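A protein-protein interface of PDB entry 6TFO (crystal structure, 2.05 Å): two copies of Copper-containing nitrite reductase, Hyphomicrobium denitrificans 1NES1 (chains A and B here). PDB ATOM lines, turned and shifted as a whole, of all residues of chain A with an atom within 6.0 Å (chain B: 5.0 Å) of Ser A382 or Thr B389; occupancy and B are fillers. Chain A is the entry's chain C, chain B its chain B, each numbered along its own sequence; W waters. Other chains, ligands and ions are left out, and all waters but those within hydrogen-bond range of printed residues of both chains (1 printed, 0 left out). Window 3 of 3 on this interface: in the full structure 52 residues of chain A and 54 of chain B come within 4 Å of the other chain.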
ATOM      1  N   VAL A 255      16.065 -12.492   4.525  1.00  0.00           N
ATOM      2  CA  VAL A 255      17.359 -12.306   5.247  1.00  0.00           C
ATOM      3  C   VAL A 255      17.500 -13.366   6.320  1.00  0.00           C
ATOM      4  O   VAL A 255      16.593 -13.559   7.112  1.00  0.00           O
ATOM      5  CB  VAL A 255      17.468 -10.907   5.861  1.00  0.00           C
ATOM      6  CG1 VAL A 255      18.826 -10.717   6.514  1.00  0.00           C
ATOM      7  CG2 VAL A 255      17.177  -9.824   4.826  1.00  0.00           C
ATOM      8  N   PRO A 256      18.629 -14.102   6.358  1.00  0.00           N
ATOM      9  CA  PRO A 256      18.887 -15.039   7.440  1.00  0.00           C
ATOM     10  C   PRO A 256      19.227 -14.253   8.710  1.00  0.00           C
ATOM     11  O   PRO A 256      19.803 -13.169   8.621  1.00  0.00           O
ATOM     12  CB  PRO A 256      20.106 -15.858   6.988  1.00  0.00           C
ATOM     13  CG  PRO A 256      20.373 -15.429   5.564  1.00  0.00           C
ATOM     14  CD  PRO A 256      19.735 -14.069   5.389  1.00  0.00           C
ATOM     15  N   GLY A 257      18.882 -14.843   9.847  1.00  0.00           N
ATOM     16  CA  GLY A 257      18.920 -14.190  11.163  1.00  0.00           C
ATOM     17  C   GLY A 257      18.035 -14.890  12.175  1.00  0.00           C
ATOM     18  O   GLY A 257      17.218 -15.749  11.780  1.00  0.00           O
ATOM     19  N   ILE A 258      18.245 -14.557  13.447  1.00  0.00           N
ATOM     20  CA  ILE A 258      17.405 -15.000  14.594  1.00  0.00           C
ATOM     21  C   ILE A 258      16.606 -13.763  15.040  1.00  0.00           C
ATOM     22  O   ILE A 258      17.185 -12.791  15.540  1.00  0.00           O
ATOM     23  CB  ILE A 258      18.265 -15.686  15.679  1.00  0.00           C
ATOM     24  CG1 ILE A 258      17.404 -16.164  16.848  1.00  0.00           C
ATOM     25  CG2 ILE A 258      19.437 -14.819  16.134  1.00  0.00           C
ATOM     26  CD1 ILE A 258      16.381 -17.193  16.462  1.00  0.00           C
ATOM     27  N   TYR A 378      26.708 -15.039  18.285  1.00  0.00           N
ATOM     28  CA  TYR A 378      26.276 -14.408  17.014  1.00  0.00           C
ATOM     29  C   TYR A 378      25.856 -12.982  17.367  1.00  0.00           C
ATOM     30  O   TYR A 378      24.718 -12.774  17.795  1.00  0.00           O
ATOM     31  CB  TYR A 378      25.232 -15.304  16.344  1.00  0.00           C
ATOM     32  CG  TYR A 378      25.784 -16.611  15.812  1.00  0.00           C
ATOM     33  CD1 TYR A 378      26.262 -17.595  16.664  1.00  0.00           C
ATOM     34  CD2 TYR A 378      25.883 -16.843  14.451  1.00  0.00           C
ATOM     35  CE1 TYR A 378      26.776 -18.788  16.187  1.00  0.00           C
ATOM     36  CE2 TYR A 378      26.392 -18.028  13.953  1.00  0.00           C
ATOM     37  CZ  TYR A 378      26.839 -19.003  14.823  1.00  0.00           C
ATOM     38  OH  TYR A 378      27.358 -20.156  14.310  1.00  0.00           O
ATOM     39  N   ALA A 379      26.793 -12.037  17.291  1.00  0.00           N
ATOM     40  CA  ALA A 379      26.649 -10.639  17.748  1.00  0.00           C
ATOM     41  C   ALA A 379      25.466  -9.991  17.016  1.00  0.00           C
ATOM     42  O   ALA A 379      25.402 -10.078  15.740  1.00  0.00           O
ATOM     43  CB  ALA A 379      27.925  -9.864  17.524  1.00  0.00           C
ATOM     44  N   LEU A 380      24.563  -9.399  17.806  1.00  0.00           N
ATOM     45  CA  LEU A 380      23.367  -8.651  17.347  1.00  0.00           C
ATOM     46  C   LEU A 380      22.470  -9.591  16.543  1.00  0.00           C
ATOM     47  O   LEU A 380      21.626  -9.097  15.785  1.00  0.00           O
ATOM     48  CB  LEU A 380      23.817  -7.416  16.555  1.00  0.00           C
ATOM     49  CG  LEU A 380      24.715  -6.448  17.338  1.00  0.00           C
ATOM     50  CD1 LEU A 380      25.102  -5.233  16.499  1.00  0.00           C
ATOM     51  CD2 LEU A 380      24.025  -5.978  18.619  1.00  0.00           C
ATOM     52  N   GLY A 381      22.619 -10.900  16.768  1.00  0.00           N
ATOM     53  CA  GLY A 381      21.836 -11.952  16.091  1.00  0.00           C
ATOM     54  C   GLY A 381      22.161 -12.077  14.608  1.00  0.00           C
ATOM     55  O   GLY A 381      21.277 -12.574  13.849  1.00  0.00           O
ATOM     56  N   SER A 382      23.361 -11.637  14.196  1.00  0.00           N
ATOM     57  CA  SER A 382      23.852 -11.837  12.809  1.00  0.00           C
ATOM     58  C   SER A 382      24.235 -13.300  12.644  1.00  0.00           C
ATOM     59  O   SER A 382      25.066 -13.818  13.419  1.00  0.00           O
ATOM     60  CB  SER A 382      24.979 -10.946  12.420  1.00  0.00           C
ATOM     61  OG  SER A 382      25.311 -11.189  11.058  1.00  0.00           O
ATOM     62  N   VAL A 383      23.580 -13.947  11.694  1.00  0.00           N
ATOM     63  CA  VAL A 383      23.784 -15.383  11.383  1.00  0.00           C
ATOM     64  C   VAL A 383      24.733 -15.441  10.175  1.00  0.00           C
ATOM     65  O   VAL A 383      25.269 -16.496   9.915  1.00  0.00           O
ATOM     66  CB  VAL A 383      22.394 -16.005  11.182  1.00  0.00           C
ATOM     67  CG1 VAL A 383      22.261 -16.842   9.923  1.00  0.00           C
ATOM     68  CG2 VAL A 383      21.964 -16.771  12.412  1.00  0.00           C
ATOM     69  N   THR A 384      25.013 -14.297   9.539  1.00  0.00           N
ATOM     70  CA  THR A 384      25.804 -14.203   8.288  1.00  0.00           C
ATOM     71  C   THR A 384      27.216 -13.700   8.598  1.00  0.00           C
ATOM     72  O   THR A 384      28.132 -14.147   7.899  1.00  0.00           O
ATOM     73  CB  THR A 384      25.079 -13.348   7.249  1.00  0.00           C
ATOM     74  OG1 THR A 384      24.750 -12.066   7.780  1.00  0.00           O
ATOM     75  CG2 THR A 384      23.796 -13.995   6.775  1.00  0.00           C
ATOM     76  N   SER A 385      27.402 -12.861   9.619  1.00  0.00           N
ATOM     77  CA  SER A 385      28.742 -12.436  10.077  1.00  0.00           C
ATOM     78  C   SER A 385      29.378 -13.528  10.931  1.00  0.00           C
ATOM     79  O   SER A 385      28.698 -14.312  11.587  1.00  0.00           O
ATOM     80  CB  SER A 385      28.689 -11.140  10.800  1.00  0.00           C
ATOM     81  OG  SER A 385      28.320 -10.090   9.915  1.00  0.00           O
ATOM     82  N   PRO A 386      30.722 -13.648  10.894  1.00  0.00           N
ATOM     83  CA  PRO A 386      31.414 -14.647  11.693  1.00  0.00           C
ATOM     84  C   PRO A 386      31.109 -14.382  13.155  1.00  0.00           C
ATOM     85  O   PRO A 386      31.158 -13.240  13.603  1.00  0.00           O
ATOM     86  CB  PRO A 386      32.906 -14.465  11.379  1.00  0.00           C
ATOM     87  CG  PRO A 386      33.007 -13.115  10.676  1.00  0.00           C
ATOM     88  CD  PRO A 386      31.645 -12.855  10.066  1.00  0.00           C
ATOM     89  N   PRO A 387      30.771 -15.426  13.933  1.00  0.00           N
ATOM     90  CA  PRO A 387      30.531 -15.244  15.362  1.00  0.00           C
ATOM     91  C   PRO A 387      31.796 -14.853  16.130  1.00  0.00           C
ATOM     92  O   PRO A 387      32.877 -15.189  15.701  1.00  0.00           O
ATOM     93  CB  PRO A 387      29.989 -16.603  15.811  1.00  0.00           C
ATOM     94  CG  PRO A 387      30.481 -17.581  14.757  1.00  0.00           C
ATOM     95  CD  PRO A 387      30.561 -16.801  13.462  1.00  0.00           C
ATOM     96  N   ALA A 401      17.827 -10.512  19.590  1.00  0.00           N
ATOM     97  CA  ALA A 401      18.111 -11.929  19.893  1.00  0.00           C
ATOM     98  C   ALA A 401      19.543 -12.207  19.463  1.00  0.00           C
ATOM     99  O   ALA A 401      20.128 -11.369  18.781  1.00  0.00           O
ATOM    100  CB  ALA A 401      17.128 -12.835  19.186  1.00  0.00           C
ATOM    101  N   PHE B 374      18.441  -4.431   8.958  1.00  0.00           N
ATOM    102  CA  PHE B 374      19.683  -3.695   8.631  1.00  0.00           C
ATOM    103  C   PHE B 374      20.558  -4.618   7.772  1.00  0.00           C
ATOM    104  O   PHE B 374      20.920  -5.714   8.251  1.00  0.00           O
ATOM    105  CB  PHE B 374      20.350  -3.200   9.917  1.00  0.00           C
ATOM    106  CG  PHE B 374      19.493  -2.253  10.718  1.00  0.00           C
ATOM    107  CD1 PHE B 374      18.730  -1.273  10.092  1.00  0.00           C
ATOM    108  CD2 PHE B 374      19.460  -2.327  12.096  1.00  0.00           C
ATOM    109  CE1 PHE B 374      17.949  -0.396  10.826  1.00  0.00           C
ATOM    110  CE2 PHE B 374      18.680  -1.444  12.827  1.00  0.00           C
ATOM    111  CZ  PHE B 374      17.922  -0.485  12.190  1.00  0.00           C
ATOM    112  N   ASP B 375      20.829  -4.224   6.528  1.00  0.00           N
ATOM    113  CA  ASP B 375      21.739  -5.005   5.647  1.00  0.00           C
ATOM    114  C   ASP B 375      23.116  -4.979   6.299  1.00  0.00           C
ATOM    115  O   ASP B 375      23.685  -6.061   6.490  1.00  0.00           O
ATOM    116  CB  ASP B 375      21.741  -4.480   4.215  1.00  0.00           C
ATOM    117  CG  ASP B 375      20.465  -4.821   3.473  1.00  0.00           C
ATOM    118  OD1 ASP B 375      19.797  -5.806   3.873  1.00  0.00           O
ATOM    119  OD2 ASP B 375      20.142  -4.082   2.519  1.00  0.00           O
ATOM    120  N   HIS B 376      23.557  -3.783   6.697  1.00  0.00           N
ATOM    121  CA  HIS B 376      24.863  -3.514   7.350  1.00  0.00           C
ATOM    122  C   HIS B 376      24.641  -2.693   8.625  1.00  0.00           C
ATOM    123  O   HIS B 376      23.838  -1.734   8.588  1.00  0.00           O
ATOM    124  CB  HIS B 376      25.803  -2.800   6.365  1.00  0.00           C
ATOM    125  CG  HIS B 376      26.031  -3.583   5.113  1.00  0.00           C
ATOM    126  ND1 HIS B 376      25.336  -3.329   3.955  1.00  0.00           N
ATOM    127  CD2 HIS B 376      26.813  -4.659   4.859  1.00  0.00           C
ATOM    128  CE1 HIS B 376      25.702  -4.185   3.027  1.00  0.00           C
ATOM    129  NE2 HIS B 376      26.602  -5.012   3.559  1.00  0.00           N
ATOM    130  N   PRO B 387      31.282  -4.342   8.744  1.00  0.00           N
ATOM    131  CA  PRO B 387      29.947  -4.269   9.325  1.00  0.00           C
ATOM    132  C   PRO B 387      29.312  -5.651   9.524  1.00  0.00           C
ATOM    133  O   PRO B 387      29.638  -6.553   8.826  1.00  0.00           O
ATOM    134  CB  PRO B 387      29.148  -3.420   8.324  1.00  0.00           C
ATOM    135  CG  PRO B 387      29.916  -3.584   7.015  1.00  0.00           C
ATOM    136  CD  PRO B 387      31.369  -3.701   7.426  1.00  0.00           C
ATOM    137  N   LEU B 388      28.437  -5.756  10.523  1.00  0.00           N
ATOM    138  CA  LEU B 388      27.610  -6.951  10.794  1.00  0.00           C
ATOM    139  C   LEU B 388      26.442  -6.923   9.817  1.00  0.00           C
ATOM    140  O   LEU B 388      26.143  -5.828   9.286  1.00  0.00           O
ATOM    141  CB  LEU B 388      27.177  -6.935  12.261  1.00  0.00           C
ATOM    142  CG  LEU B 388      28.328  -7.136  13.257  1.00  0.00           C
ATOM    143  CD1 LEU B 388      27.975  -6.588  14.627  1.00  0.00           C
ATOM    144  CD2 LEU B 388      28.721  -8.597  13.370  1.00  0.00           C
ATOM    145  N   THR B 389      25.862  -8.083   9.522  1.00  0.00           N
ATOM    146  CA  THR B 389      24.924  -8.229   8.380  1.00  0.00           C
ATOM    147  C   THR B 389      23.632  -8.908   8.843  1.00  0.00           C
ATOM    148  O   THR B 389      23.709  -9.865   9.659  1.00  0.00           O
ATOM    149  CB  THR B 389      25.608  -8.971   7.223  1.00  0.00           C
ATOM    150  OG1 THR B 389      26.211 -10.165   7.732  1.00  0.00           O
ATOM    151  CG2 THR B 389      26.652  -8.114   6.538  1.00  0.00           C
ATOM    152  N   GLY B 390      22.495  -8.449   8.315  1.00  0.00           N
ATOM    153  CA  GLY B 390      21.183  -9.054   8.611  1.00  0.00           C
ATOM    154  C   GLY B 390      20.872  -8.938  10.092  1.00  0.00           C
ATOM    155  O   GLY B 390      20.743  -9.999  10.757  1.00  0.00           O
ATOM    156  N   VAL B 391      20.800  -7.689  10.583  1.00  0.00           N
ATOM    157  CA  VAL B 391      20.631  -7.311  12.023  1.00  0.00           C
ATOM    158  C   VAL B 391      19.288  -6.588  12.195  1.00  0.00           C
ATOM    159  O   VAL B 391      19.076  -5.576  11.506  1.00  0.00           O
ATOM    160  CB  VAL B 391      21.811  -6.446  12.519  1.00  0.00           C
ATOM    161  CG1 VAL B 391      21.538  -5.789  13.875  1.00  0.00           C
ATOM    162  CG2 VAL B 391      23.093  -7.255  12.583  1.00  0.00           C
HETATM  163  O   HOH W   1      19.391 -11.506  12.356  1.00  0.00           O
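The side-chain hydroxyl (OG) of Ser A382 sits at hydrogen-bond distance from the backbone carbonyl oxygen (O) of Thr B389 (2.5 Å).
The side-chain hydroxyl (OG1) of Thr A384 sits at hydrogen-bond distance from the backbone carbonyl oxygen (O) of Thr B389, 3.1 Å away.
The side-chain hydroxyl of Thr B389 lies within hydrogen-bond range of the side-chain hydroxyl of Ser A385 (3.0 Å).
The backbone NH of Gly B390 sits at hydrogen-bond distance from the backbone carbonyl oxygen of Phe B374, 3.2 Å away.
N of Phe B374 is in hydrogen-bond range of O of Val B391, at 2.9 Å.
O of Asp B375 lies within hydrogen-bond range of N of Gly B390.
The side-chain hydroxyl (OG) of Ser A382 sits at hydrogen-bond distance from the side-chain hydroxyl (OG1) of Thr A384 (3.4 Å).
The side-chain hydroxyl of Ser A382 sits at hydrogen-bond distance from the backbone NH of Ser A385 (3.0 Å).
Among the printed residues, merely in contact across the chains: Val A255 with Gly B390 (3.6 Å), Pro A256 with Gly B390 (3.9 Å), Leu A380 with Leu B388 (3.7 Å), Leu A380 with Val B391 (3.8 Å), Ser A385 with Pro B387 (3.9 Å) and Ser A385 with Leu B388 (3.3 Å).
Of the printed residues of chain B, Pro A256 touches Gly B390 (3.9 Å).
Ile A258 touches none of the printed residues of chain B.
Of the printed residues of chain B, Leu A380 touches Leu B388 (3.7 Å) and Val B391 (3.8 Å).
Printed residues of chain B within 4 Å of Thr A384: Thr B389.
Printed residues of chain A within 4 Å of Pro B387: Ser A385.
Printed residues of chain A within 4 Å of Leu B388: Leu A380 (3.7 Å) and Ser A385 (3.3 Å).
Thr B389 touches just these residues of chain A: Ser A382 (2.5 Å), Thr A384 (2.4 Å) and Ser A385 (3.0 Å).
The nearest printed residue of chain B that does not touch Ser A382 is Val B391 (4.1 Å).
Hydrophobic or aromatic side chains of chain A that line the printed part of chain B: Val A255 and Leu A380.
Along chain A the printed residues that touch a printed residue of chain B span positions 255 to 385.
Of the 8 printed residues of chain B, 5 touch a printed residue of chain A.
Hydrophobic or aromatic side chains of chain B within 4 Å of the printed part of chain A: Leu B388 and Val B391.
Among the printed residues, 9 pairs touch across the chains.
Position printed for both chains: 387.
Of the 9 pairs that touch across the chains among the printed residues, none has its exchanged pair printed and touching as well.
Water W1 lies within hydrogen-bond range of the backbone carbonyl oxygen of Gly B390 (2.6 Å), the backbone carbonyl oxygen of Gly A381 (2.6 Å) and the backbone NH of Ile A258 (3.4 Å).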
